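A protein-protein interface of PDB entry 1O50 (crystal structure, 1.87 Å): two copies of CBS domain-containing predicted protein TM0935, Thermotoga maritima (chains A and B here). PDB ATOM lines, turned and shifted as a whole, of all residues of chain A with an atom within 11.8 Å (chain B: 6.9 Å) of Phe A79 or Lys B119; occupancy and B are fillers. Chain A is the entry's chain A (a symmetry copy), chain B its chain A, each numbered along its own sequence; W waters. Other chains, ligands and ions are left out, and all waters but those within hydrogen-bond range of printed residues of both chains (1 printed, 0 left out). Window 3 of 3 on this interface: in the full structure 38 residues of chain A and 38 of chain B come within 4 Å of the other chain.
Of chain B, only Lys B119, Ile B122 and Asp B123 come within 4 Å of Phe A79.
No residue of chain A comes within 4 Å of Ala B117.
Leu B120 touches none of the printed residues of chain A.
Ile B122 touches just these residues of chain A: Phe A79 (3.9 Å) and Pro A81 (3.7 Å).
Of the printed residues of chain B, Gly A73 touches Leu B118.
Printed residues of chain A within 4 Å of Glu B115: Phe A77 (3.7 Å).
No position is printed for both chains.
Among the printed residues, merely in contact across the chains: Met A66 with Asn B125, Gly A73 with Leu B118, Phe A77 with Glu B115, Phe A79 with Lys B119, Phe A79 with Ile B122, Phe A79 with Asp B123 and Pro A81 with Ile B122.
Hydrophobic or aromatic side chains of chain A that line the printed part of chain B: Met A66, Phe A77, Phe A79 and Pro A81.
The side-chain carboxylate of Asp B123 is in salt-bridge range of the side-chain amino group of Lys B119 (3.4 Å).
O of Gly A73 is in hydrogen-bond range of N of Gly A78, 3.1 Å away.
O of Gly A73 lies within hydrogen-bond range of N of Phe A79, 3.0 Å away.
Water W1 lies within hydrogen-bond range of the backbone carbonyl oxygen (O) of Ile B122 (3.1 Å), the side-chain amino group (NZ) of Lys A70 (3.3 Å) and the side-chain amide oxygen (OD1) of Asn B125 (3.4 Å).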
ATOM      1  N   MET A  66       5.595  29.228   7.458  1.00  0.00           N
ATOM      2  CA  MET A  66       6.957  29.212   8.013  1.00  0.00           C
ATOM      3  C   MET A  66       7.012  30.137   9.233  1.00  0.00           C
ATOM      4  O   MET A  66       7.846  29.936  10.165  1.00  0.00           O
ATOM      5  CB  MET A  66       8.006  29.605   6.960  1.00  0.00           C
ATOM      6  CG  MET A  66       9.425  29.862   7.534  1.00  0.00           C
ATOM      7  SD  MET A  66      10.258  28.314   8.264  1.00  0.00           S
ATOM      8  CE  MET A  66      10.797  27.553   6.818  1.00  0.00           C
ATOM      9  N   HIS A  67       6.195  31.190   9.228  1.00  0.00           N
ATOM     10  CA  HIS A  67       6.109  32.038  10.422  1.00  0.00           C
ATOM     11  C   HIS A  67       5.517  31.222  11.616  1.00  0.00           C
ATOM     12  O   HIS A  67       6.041  31.286  12.709  1.00  0.00           O
ATOM     13  CB  HIS A  67       5.290  33.291  10.170  1.00  0.00           C
ATOM     14  CG  HIS A  67       5.174  34.193  11.366  1.00  0.00           C
ATOM     15  ND1 HIS A  67       6.267  34.751  12.002  1.00  0.00           N
ATOM     16  CD2 HIS A  67       4.079  34.689  11.994  1.00  0.00           C
ATOM     17  CE1 HIS A  67       5.843  35.541  12.982  1.00  0.00           C
ATOM     18  NE2 HIS A  67       4.516  35.497  13.012  1.00  0.00           N
ATOM     19  N   LEU A  68       4.482  30.424  11.364  1.00  0.00           N
ATOM     20  CA  LEU A  68       3.850  29.566  12.370  1.00  0.00           C
ATOM     21  C   LEU A  68       4.826  28.506  12.893  1.00  0.00           C
ATOM     22  O   LEU A  68       4.857  28.192  14.096  1.00  0.00           O
ATOM     23  CB  LEU A  68       2.602  28.891  11.771  1.00  0.00           C
ATOM     24  CG  LEU A  68       1.713  28.061  12.696  1.00  0.00           C
ATOM     25  CD1 LEU A  68       1.393  28.785  14.010  1.00  0.00           C
ATOM     26  CD2 LEU A  68       0.409  27.647  11.970  1.00  0.00           C
ATOM     27  N   LEU A  69       5.667  27.997  11.994  1.00  0.00           N
ATOM     28  CA  LEU A  69       6.690  27.024  12.350  1.00  0.00           C
ATOM     29  C   LEU A  69       7.711  27.695  13.288  1.00  0.00           C
ATOM     30  O   LEU A  69       8.099  27.122  14.301  1.00  0.00           O
ATOM     31  CB  LEU A  69       7.365  26.502  11.077  1.00  0.00           C
ATOM     32  CG  LEU A  69       8.290  25.304  11.216  1.00  0.00           C
ATOM     33  CD1 LEU A  69       7.455  24.062  11.607  1.00  0.00           C
ATOM     34  CD2 LEU A  69       9.129  25.037   9.950  1.00  0.00           C
ATOM     35  N   LYS A  70       8.089  28.930  12.985  1.00  0.00           N
ATOM     36  CA  LYS A  70       9.056  29.657  13.775  1.00  0.00           C
ATOM     37  C   LYS A  70       8.486  29.987  15.176  1.00  0.00           C
ATOM     38  O   LYS A  70       9.146  29.801  16.192  1.00  0.00           O
ATOM     39  CB  LYS A  70       9.535  30.931  13.044  1.00  0.00           C
ATOM     40  CG  LYS A  70      10.500  30.653  11.903  1.00  0.00           C
ATOM     41  CD  LYS A  70      10.807  31.924  11.131  1.00  0.00           C
ATOM     42  CE  LYS A  70      11.682  31.651   9.902  1.00  0.00           C
ATOM     43  NZ  LYS A  70      11.914  32.924   9.075  1.00  0.00           N
ATOM     44  N   VAL A  71       7.261  30.488  15.191  1.00  0.00           N
ATOM     45  CA  VAL A  71       6.525  30.781  16.417  1.00  0.00           C
ATOM     46  C   VAL A  71       6.474  29.503  17.284  1.00  0.00           C
ATOM     47  O   VAL A  71       6.617  29.556  18.507  1.00  0.00           O
ATOM     48  CB  VAL A  71       5.091  31.291  16.038  1.00  0.00           C
ATOM     49  CG1 VAL A  71       4.134  31.125  17.185  1.00  0.00           C
ATOM     50  CG2 VAL A  71       5.158  32.730  15.577  1.00  0.00           C
ATOM     51  N   SER A  72       6.279  28.358  16.627  1.00  0.00           N
ATOM     52  CA  SER A  72       6.112  27.077  17.295  1.00  0.00           C
ATOM     53  C   SER A  72       7.418  26.602  17.890  1.00  0.00           C
ATOM     54  O   SER A  72       7.427  26.211  19.027  1.00  0.00           O
ATOM     55  CB  SER A  72       5.500  26.021  16.370  1.00  0.00           C
ATOM     56  OG  SER A  72       4.275  26.504  15.854  1.00  0.00           O
ATOM     57  N   GLY A  73       8.527  26.684  17.157  1.00  0.00           N
ATOM     58  CA  GLY A  73       9.826  26.340  17.676  1.00  0.00           C
ATOM     59  C   GLY A  73      10.263  27.134  18.883  1.00  0.00           C
ATOM     60  O   GLY A  73      10.963  26.607  19.752  1.00  0.00           O
ATOM     61  N   PHE A  74       9.943  28.434  18.920  1.00  0.00           N
ATOM     62  CA  PHE A  74      10.190  29.240  20.091  1.00  0.00           C
ATOM     63  C   PHE A  74       9.302  28.811  21.278  1.00  0.00           C
ATOM     64  O   PHE A  74       9.772  28.598  22.369  1.00  0.00           O
ATOM     65  CB  PHE A  74       9.985  30.725  19.804  1.00  0.00           C
ATOM     66  CG  PHE A  74      10.221  31.568  20.992  1.00  0.00           C
ATOM     67  CD1 PHE A  74      11.495  31.713  21.489  1.00  0.00           C
ATOM     68  CD2 PHE A  74       9.158  32.172  21.660  1.00  0.00           C
ATOM     69  CE1 PHE A  74      11.749  32.485  22.636  1.00  0.00           C
ATOM     70  CE2 PHE A  74       9.374  32.932  22.788  1.00  0.00           C
ATOM     71  CZ  PHE A  74      10.675  33.108  23.286  1.00  0.00           C
ATOM     72  N   HIS A  75       8.000  28.670  21.035  1.00  0.00           N
ATOM     73  CA  HIS A  75       7.076  28.362  22.104  1.00  0.00           C
ATOM     74  C   HIS A  75       7.364  27.003  22.749  1.00  0.00           C
ATOM     75  O   HIS A  75       7.321  26.885  23.960  1.00  0.00           O
ATOM     76  CB  HIS A  75       5.636  28.333  21.556  1.00  0.00           C
ATOM     77  CG  HIS A  75       4.607  28.100  22.614  1.00  0.00           C
ATOM     78  ND1 HIS A  75       4.272  29.061  23.542  1.00  0.00           N
ATOM     79  CD2 HIS A  75       3.837  27.019  22.891  1.00  0.00           C
ATOM     80  CE1 HIS A  75       3.331  28.584  24.339  1.00  0.00           C
ATOM     81  NE2 HIS A  75       3.062  27.347  23.976  1.00  0.00           N
ATOM     82  N   PHE A  76       7.625  25.981  21.926  1.00  0.00           N
ATOM     83  CA  PHE A  76       7.784  24.615  22.415  1.00  0.00           C
ATOM     84  C   PHE A  76       9.222  24.222  22.734  1.00  0.00           C
ATOM     85  O   PHE A  76       9.442  23.411  23.620  1.00  0.00           O
ATOM     86  CB  PHE A  76       7.169  23.638  21.426  1.00  0.00           C
ATOM     87  CG  PHE A  76       5.681  23.670  21.418  1.00  0.00           C
ATOM     88  CD1 PHE A  76       4.963  23.068  22.441  1.00  0.00           C
ATOM     89  CD2 PHE A  76       4.980  24.287  20.407  1.00  0.00           C
ATOM     90  CE1 PHE A  76       3.594  23.112  22.447  1.00  0.00           C
ATOM     91  CE2 PHE A  76       3.630  24.303  20.405  1.00  0.00           C
ATOM     92  CZ  PHE A  76       2.934  23.730  21.447  1.00  0.00           C
ATOM     93  N   PHE A  77      10.195  24.804  22.032  1.00  0.00           N
ATOM     94  CA  PHE A  77      11.625  24.412  22.203  1.00  0.00           C
ATOM     95  C   PHE A  77      12.532  25.554  22.593  1.00  0.00           C
ATOM     96  O   PHE A  77      13.735  25.340  22.806  1.00  0.00           O
ATOM     97  CB  PHE A  77      12.178  23.784  20.907  1.00  0.00           C
ATOM     98  CG  PHE A  77      11.426  22.571  20.444  1.00  0.00           C
ATOM     99  CD1 PHE A  77      11.425  21.409  21.200  1.00  0.00           C
ATOM    100  CD2 PHE A  77      10.704  22.597  19.264  1.00  0.00           C
ATOM    101  CE1 PHE A  77      10.719  20.299  20.764  1.00  0.00           C
ATOM    102  CE2 PHE A  77      10.020  21.501  18.846  1.00  0.00           C
ATOM    103  CZ  PHE A  77      10.017  20.356  19.593  1.00  0.00           C
ATOM    104  N   GLY A  78      11.995  26.767  22.680  1.00  0.00           N
ATOM    105  CA  GLY A  78      12.837  27.959  22.884  1.00  0.00           C
ATOM    106  C   GLY A  78      13.848  28.324  21.798  1.00  0.00           C
ATOM    107  O   GLY A  78      14.851  28.932  22.082  1.00  0.00           O
ATOM    108  N   PHE A  79      13.584  27.920  20.571  1.00  0.00           N
ATOM    109  CA  PHE A  79      14.445  28.158  19.411  1.00  0.00           C
ATOM    110  C   PHE A  79      14.235  29.570  18.844  1.00  0.00           C
ATOM    111  O   PHE A  79      13.121  29.951  18.468  1.00  0.00           O
ATOM    112  CB  PHE A  79      14.199  27.075  18.310  1.00  0.00           C
ATOM    113  CG  PHE A  79      15.185  27.137  17.168  1.00  0.00           C
ATOM    114  CD1 PHE A  79      16.563  26.931  17.407  1.00  0.00           C
ATOM    115  CD2 PHE A  79      14.777  27.435  15.868  1.00  0.00           C
ATOM    116  CE1 PHE A  79      17.497  27.029  16.368  1.00  0.00           C
ATOM    117  CE2 PHE A  79      15.722  27.527  14.827  1.00  0.00           C
ATOM    118  CZ  PHE A  79      17.066  27.339  15.088  1.00  0.00           C
ATOM    119  N   ILE A  80      15.308  30.340  18.799  1.00  0.00           N
ATOM    120  CA  ILE A  80      15.308  31.649  18.145  1.00  0.00           C
ATOM    121  C   ILE A  80      16.023  31.532  16.785  1.00  0.00           C
ATOM    122  O   ILE A  80      17.190  31.208  16.765  1.00  0.00           O
ATOM    123  CB  ILE A  80      16.013  32.655  19.029  1.00  0.00           C
ATOM    124  CG1 ILE A  80      15.274  32.748  20.371  1.00  0.00           C
ATOM    125  CG2 ILE A  80      16.100  34.030  18.317  1.00  0.00           C
ATOM    126  CD1 ILE A  80      16.141  33.271  21.517  1.00  0.00           C
ATOM    127  N   PRO A  81      15.317  31.703  15.658  1.00  0.00           N
ATOM    128  CA  PRO A  81      15.997  31.771  14.347  1.00  0.00           C
ATOM    129  C   PRO A  81      16.963  32.959  14.148  1.00  0.00           C
ATOM    130  O   PRO A  81      17.205  33.801  15.043  1.00  0.00           O
ATOM    131  CB  PRO A  81      14.828  31.866  13.363  1.00  0.00           C
ATOM    132  CG  PRO A  81      13.648  31.257  14.118  1.00  0.00           C
ATOM    133  CD  PRO A  81      13.840  31.750  15.499  1.00  0.00           C
ATOM    134  N   SER A  89      13.233  39.648  20.657  1.00  0.00           N
ATOM    135  CA  SER A  89      12.238  39.974  19.645  1.00  0.00           C
ATOM    136  C   SER A  89      10.983  39.094  19.681  1.00  0.00           C
ATOM    137  O   SER A  89       9.864  39.610  19.571  1.00  0.00           O
ATOM    138  CB  SER A  89      12.838  39.889  18.245  1.00  0.00           C
ATOM    139  OG  SER A  89      11.797  39.845  17.274  1.00  0.00           O
ATOM    140  N   MET A  90      11.142  37.769  19.763  1.00  0.00           N
ATOM    141  CA  MET A  90       9.952  36.924  19.896  1.00  0.00           C
ATOM    142  C   MET A  90       9.508  36.783  21.345  1.00  0.00           C
ATOM    143  O   MET A  90      10.319  36.674  22.268  1.00  0.00           O
ATOM    144  CB  MET A  90      10.046  35.564  19.228  1.00  0.00           C
ATOM    145  CG  MET A  90      11.411  34.958  18.999  1.00  0.00           C
ATOM    146  SD  MET A  90      11.333  33.888  17.506  1.00  0.00           S
ATOM    147  CE  MET A  90       9.383  33.592  17.162  1.00  0.00           C
ATOM    148  N   LYS A  91       8.188  36.816  21.497  1.00  0.00           N
ATOM    149  CA  LYS A  91       7.538  37.038  22.776  1.00  0.00           C
ATOM    150  C   LYS A  91       6.650  35.841  23.075  1.00  0.00           C
ATOM    151  O   LYS A  91       6.398  35.004  22.224  1.00  0.00           O
ATOM    152  CB  LYS A  91       6.723  38.338  22.749  1.00  0.00           C
ATOM    153  CG  LYS A  91       7.522  39.605  22.534  1.00  0.00           C
ATOM    154  CD  LYS A  91       8.516  39.826  23.634  1.00  0.00           C
ATOM    155  CE  LYS A  91       8.710  41.305  24.017  1.00  0.00           C
ATOM    156  NZ  LYS A  91       7.731  41.774  25.086  1.00  0.00           N
ATOM    157  N   ARG A  92       6.169  35.786  24.307  1.00  0.00           N
ATOM    158  CA  ARG A  92       5.479  34.629  24.824  1.00  0.00           C
ATOM    159  C   ARG A  92       4.037  34.634  24.334  1.00  0.00           C
ATOM    160  O   ARG A  92       3.366  35.682  24.360  1.00  0.00           O
ATOM    161  CB  ARG A  92       5.554  34.689  26.348  1.00  0.00           C
ATOM    162  CG  ARG A  92       4.782  33.625  27.074  1.00  0.00           C
ATOM    163  CD  ARG A  92       4.882  33.747  28.587  1.00  0.00           C
ATOM    164  NE  ARG A  92       4.125  32.645  29.194  1.00  0.00           N
ATOM    165  CZ  ARG A  92       4.179  32.309  30.472  1.00  0.00           C
ATOM    166  NH1 ARG A  92       4.927  32.992  31.326  1.00  0.00           N
ATOM    167  NH2 ARG A  92       3.457  31.292  30.895  1.00  0.00           N
ATOM    168  N   LEU A  93       3.544  33.467  23.925  1.00  0.00           N
ATOM    169  CA  LEU A  93       2.148  33.311  23.585  1.00  0.00           C
ATOM    170  C   LEU A  93       1.320  33.235  24.874  1.00  0.00           C
ATOM    171  O   LEU A  93       1.702  32.551  25.820  1.00  0.00           O
ATOM    172  CB  LEU A  93       1.942  32.070  22.737  1.00  0.00           C
ATOM    173  CG  LEU A  93       2.656  32.079  21.386  1.00  0.00           C
ATOM    174  CD1 LEU A  93       2.439  30.742  20.732  1.00  0.00           C
ATOM    175  CD2 LEU A  93       2.137  33.214  20.507  1.00  0.00           C
ATOM    176  N   LEU B 114      12.868  15.490  16.983  1.00  0.00           N
ATOM    177  CA  LEU B 114      11.990  16.417  16.297  1.00  0.00           C
ATOM    178  C   LEU B 114      12.539  17.863  16.307  1.00  0.00           C
ATOM    179  O   LEU B 114      12.462  18.581  15.300  1.00  0.00           O
ATOM    180  CB  LEU B 114      10.590  16.424  16.923  1.00  0.00           C
ATOM    181  CG  LEU B 114       9.518  17.184  16.157  1.00  0.00           C
ATOM    182  CD1 LEU B 114       9.292  16.510  14.795  1.00  0.00           C
ATOM    183  CD2 LEU B 114       8.201  17.205  16.952  1.00  0.00           C
ATOM    184  N   GLU B 115      13.066  18.282  17.447  1.00  0.00           N
ATOM    185  CA  GLU B 115      13.611  19.623  17.557  1.00  0.00           C
ATOM    186  C   GLU B 115      14.804  19.916  16.644  1.00  0.00           C
ATOM    187  O   GLU B 115      14.954  21.066  16.196  1.00  0.00           O
ATOM    188  CB  GLU B 115      13.967  19.959  18.995  1.00  0.00           C
ATOM    189  CG  GLU B 115      14.768  18.933  19.732  1.00  0.00           C
ATOM    190  CD  GLU B 115      15.364  19.511  21.012  1.00  0.00           C
ATOM    191  OE1 GLU B 115      16.091  18.764  21.728  1.00  0.00           O
ATOM    192  OE2 GLU B 115      15.118  20.718  21.296  1.00  0.00           O
ATOM    193  N   GLU B 116      15.661  18.917  16.405  1.00  0.00           N
ATOM    194  CA  GLU B 116      16.759  19.087  15.437  1.00  0.00           C
ATOM    195  C   GLU B 116      16.221  19.192  14.019  1.00  0.00           C
ATOM    196  O   GLU B 116      16.762  19.970  13.234  1.00  0.00           O
ATOM    197  CB  GLU B 116      17.893  18.042  15.528  1.00  0.00           C
ATOM    198  CG  GLU B 116      18.768  17.881  14.245  1.00  0.00           C
ATOM    199  CD  GLU B 116      19.720  19.054  13.846  1.00  0.00           C
ATOM    200  OE1 GLU B 116      20.844  18.764  13.332  1.00  0.00           O
ATOM    201  OE2 GLU B 116      19.381  20.255  13.999  1.00  0.00           O
ATOM    202  N   ALA B 117      15.155  18.454  13.707  1.00  0.00           N
ATOM    203  CA  ALA B 117      14.499  18.532  12.403  1.00  0.00           C
ATOM    204  C   ALA B 117      13.829  19.896  12.110  1.00  0.00           C
ATOM    205  O   ALA B 117      13.856  20.389  10.972  1.00  0.00           O
ATOM    206  CB  ALA B 117      13.493  17.427  12.277  1.00  0.00           C
ATOM    207  N   LEU B 118      13.207  20.484  13.132  1.00  0.00           N
ATOM    208  CA  LEU B 118      12.592  21.815  13.047  1.00  0.00           C
ATOM    209  C   LEU B 118      13.685  22.855  12.882  1.00  0.00           C
ATOM    210  O   LEU B 118      13.527  23.801  12.121  1.00  0.00           O
ATOM    211  CB  LEU B 118      11.731  22.102  14.306  1.00  0.00           C
ATOM    212  CG  LEU B 118      11.091  23.506  14.427  1.00  0.00           C
ATOM    213  CD1 LEU B 118       9.793  23.504  15.201  1.00  0.00           C
ATOM    214  CD2 LEU B 118      12.056  24.515  15.092  1.00  0.00           C
ATOM    215  N   LYS B 119      14.792  22.694  13.585  1.00  0.00           N
ATOM    216  CA  LYS B 119      15.918  23.613  13.467  1.00  0.00           C
ATOM    217  C   LYS B 119      16.470  23.610  12.050  1.00  0.00           C
ATOM    218  O   LYS B 119      16.750  24.650  11.494  1.00  0.00           O
ATOM    219  CB  LYS B 119      17.026  23.259  14.445  1.00  0.00           C
ATOM    220  CG  LYS B 119      18.261  24.133  14.317  1.00  0.00           C
ATOM    221  CD  LYS B 119      19.421  23.630  15.187  1.00  0.00           C
ATOM    222  CE  LYS B 119      20.720  24.368  14.870  1.00  0.00           C
ATOM    223  NZ  LYS B 119      20.726  25.764  15.398  1.00  0.00           N
ATOM    224  N   LEU B 120      16.613  22.422  11.482  1.00  0.00           N
ATOM    225  CA  LEU B 120      17.071  22.246  10.098  1.00  0.00           C
ATOM    226  C   LEU B 120      16.145  22.919   9.115  1.00  0.00           C
ATOM    227  O   LEU B 120      16.588  23.591   8.200  1.00  0.00           O
ATOM    228  CB  LEU B 120      17.159  20.743   9.744  1.00  0.00           C
ATOM    229  CG  LEU B 120      18.352  19.999  10.354  1.00  0.00           C
ATOM    230  CD1 LEU B 120      18.181  18.496  10.088  1.00  0.00           C
ATOM    231  CD2 LEU B 120      19.689  20.498   9.807  1.00  0.00           C
ATOM    232  N   MET B 121      14.855  22.705   9.273  1.00  0.00           N
ATOM    233  CA  MET B 121      13.907  23.343   8.415  1.00  0.00           C
ATOM    234  C   MET B 121      14.071  24.829   8.445  1.00  0.00           C
ATOM    235  O   MET B 121      14.171  25.467   7.407  1.00  0.00           O
ATOM    236  CB  MET B 121      12.497  23.006   8.828  1.00  0.00           C
ATOM    237  CG  MET B 121      12.092  21.640   8.408  1.00  0.00           C
ATOM    238  SD  MET B 121      10.348  21.361   8.546  1.00  0.00           S
ATOM    239  CE  MET B 121      10.435  19.637   8.350  1.00  0.00           C
ATOM    240  N   ILE B 122      14.092  25.379   9.641  1.00  0.00           N
ATOM    241  CA  ILE B 122      14.192  26.829   9.788  1.00  0.00           C
ATOM    242  C   ILE B 122      15.509  27.402   9.258  1.00  0.00           C
ATOM    243  O   ILE B 122      15.503  28.366   8.482  1.00  0.00           O
ATOM    244  CB  ILE B 122      13.924  27.236  11.239  1.00  0.00           C
ATOM    245  CG1 ILE B 122      12.435  27.014  11.558  1.00  0.00           C
ATOM    246  CG2 ILE B 122      14.237  28.730  11.414  1.00  0.00           C
ATOM    247  CD1 ILE B 122      12.091  26.967  13.050  1.00  0.00           C
ATOM    248  N   ASP B 123      16.637  26.834   9.691  1.00  0.00           N
ATOM    249  CA  ASP B 123      17.959  27.312   9.281  1.00  0.00           C
ATOM    250  C   ASP B 123      18.177  27.302   7.749  1.00  0.00           C
ATOM    251  O   ASP B 123      18.835  28.182   7.214  1.00  0.00           O
ATOM    252  CB  ASP B 123      19.068  26.460   9.935  1.00  0.00           C
ATOM    253  CG  ASP B 123      19.248  26.724  11.416  1.00  0.00           C
ATOM    254  OD1 ASP B 123      18.599  27.602  12.022  1.00  0.00           O
ATOM    255  OD2 ASP B 123      20.075  26.095  12.067  1.00  0.00           O
ATOM    256  N   ASN B 124      17.624  26.293   7.074  1.00  0.00           N
ATOM    257  CA  ASN B 124      17.755  26.073   5.628  1.00  0.00           C
ATOM    258  C   ASN B 124      16.550  26.587   4.840  1.00  0.00           C
ATOM    259  O   ASN B 124      16.475  26.500   3.602  1.00  0.00           O
ATOM    260  CB  ASN B 124      17.930  24.567   5.389  1.00  0.00           C
ATOM    261  CG  ASN B 124      19.273  24.061   5.887  1.00  0.00           C
ATOM    262  OD1 ASN B 124      20.287  24.279   5.239  1.00  0.00           O
ATOM    263  ND2 ASN B 124      19.291  23.439   7.071  1.00  0.00           N
ATOM    264  N   ASN B 125      15.597  27.137   5.563  1.00  0.00           N
ATOM    265  CA  ASN B 125      14.401  27.676   4.968  1.00  0.00           C
ATOM    266  C   ASN B 125      13.745  26.702   4.008  1.00  0.00           C
ATOM    267  O   ASN B 125      13.434  27.052   2.858  1.00  0.00           O
ATOM    268  CB  ASN B 125      14.643  29.024   4.271  1.00  0.00           C
ATOM    269  CG  ASN B 125      13.321  29.624   3.730  1.00  0.00           C
ATOM    270  OD1 ASN B 125      12.296  29.467   4.376  1.00  0.00           O
ATOM    271  ND2 ASN B 125      13.342  30.289   2.556  1.00  0.00           N
ATOM    272  N   ILE B 147       5.029  18.422  11.740  1.00  0.00           N
ATOM    273  CA  ILE B 147       5.594  18.997  12.953  1.00  0.00           C
ATOM    274  C   ILE B 147       4.551  19.837  13.648  1.00  0.00           C
ATOM    275  O   ILE B 147       4.385  19.726  14.856  1.00  0.00           O
ATOM    276  CB  ILE B 147       6.882  19.781  12.662  1.00  0.00           C
ATOM    277  CG1 ILE B 147       7.968  18.846  12.134  1.00  0.00           C
ATOM    278  CG2 ILE B 147       7.442  20.453  13.924  1.00  0.00           C
ATOM    279  CD1 ILE B 147       9.276  19.500  11.894  1.00  0.00           C
HETATM  280  O   HOH W   1      13.363  30.378   7.508  1.00  0.00           O
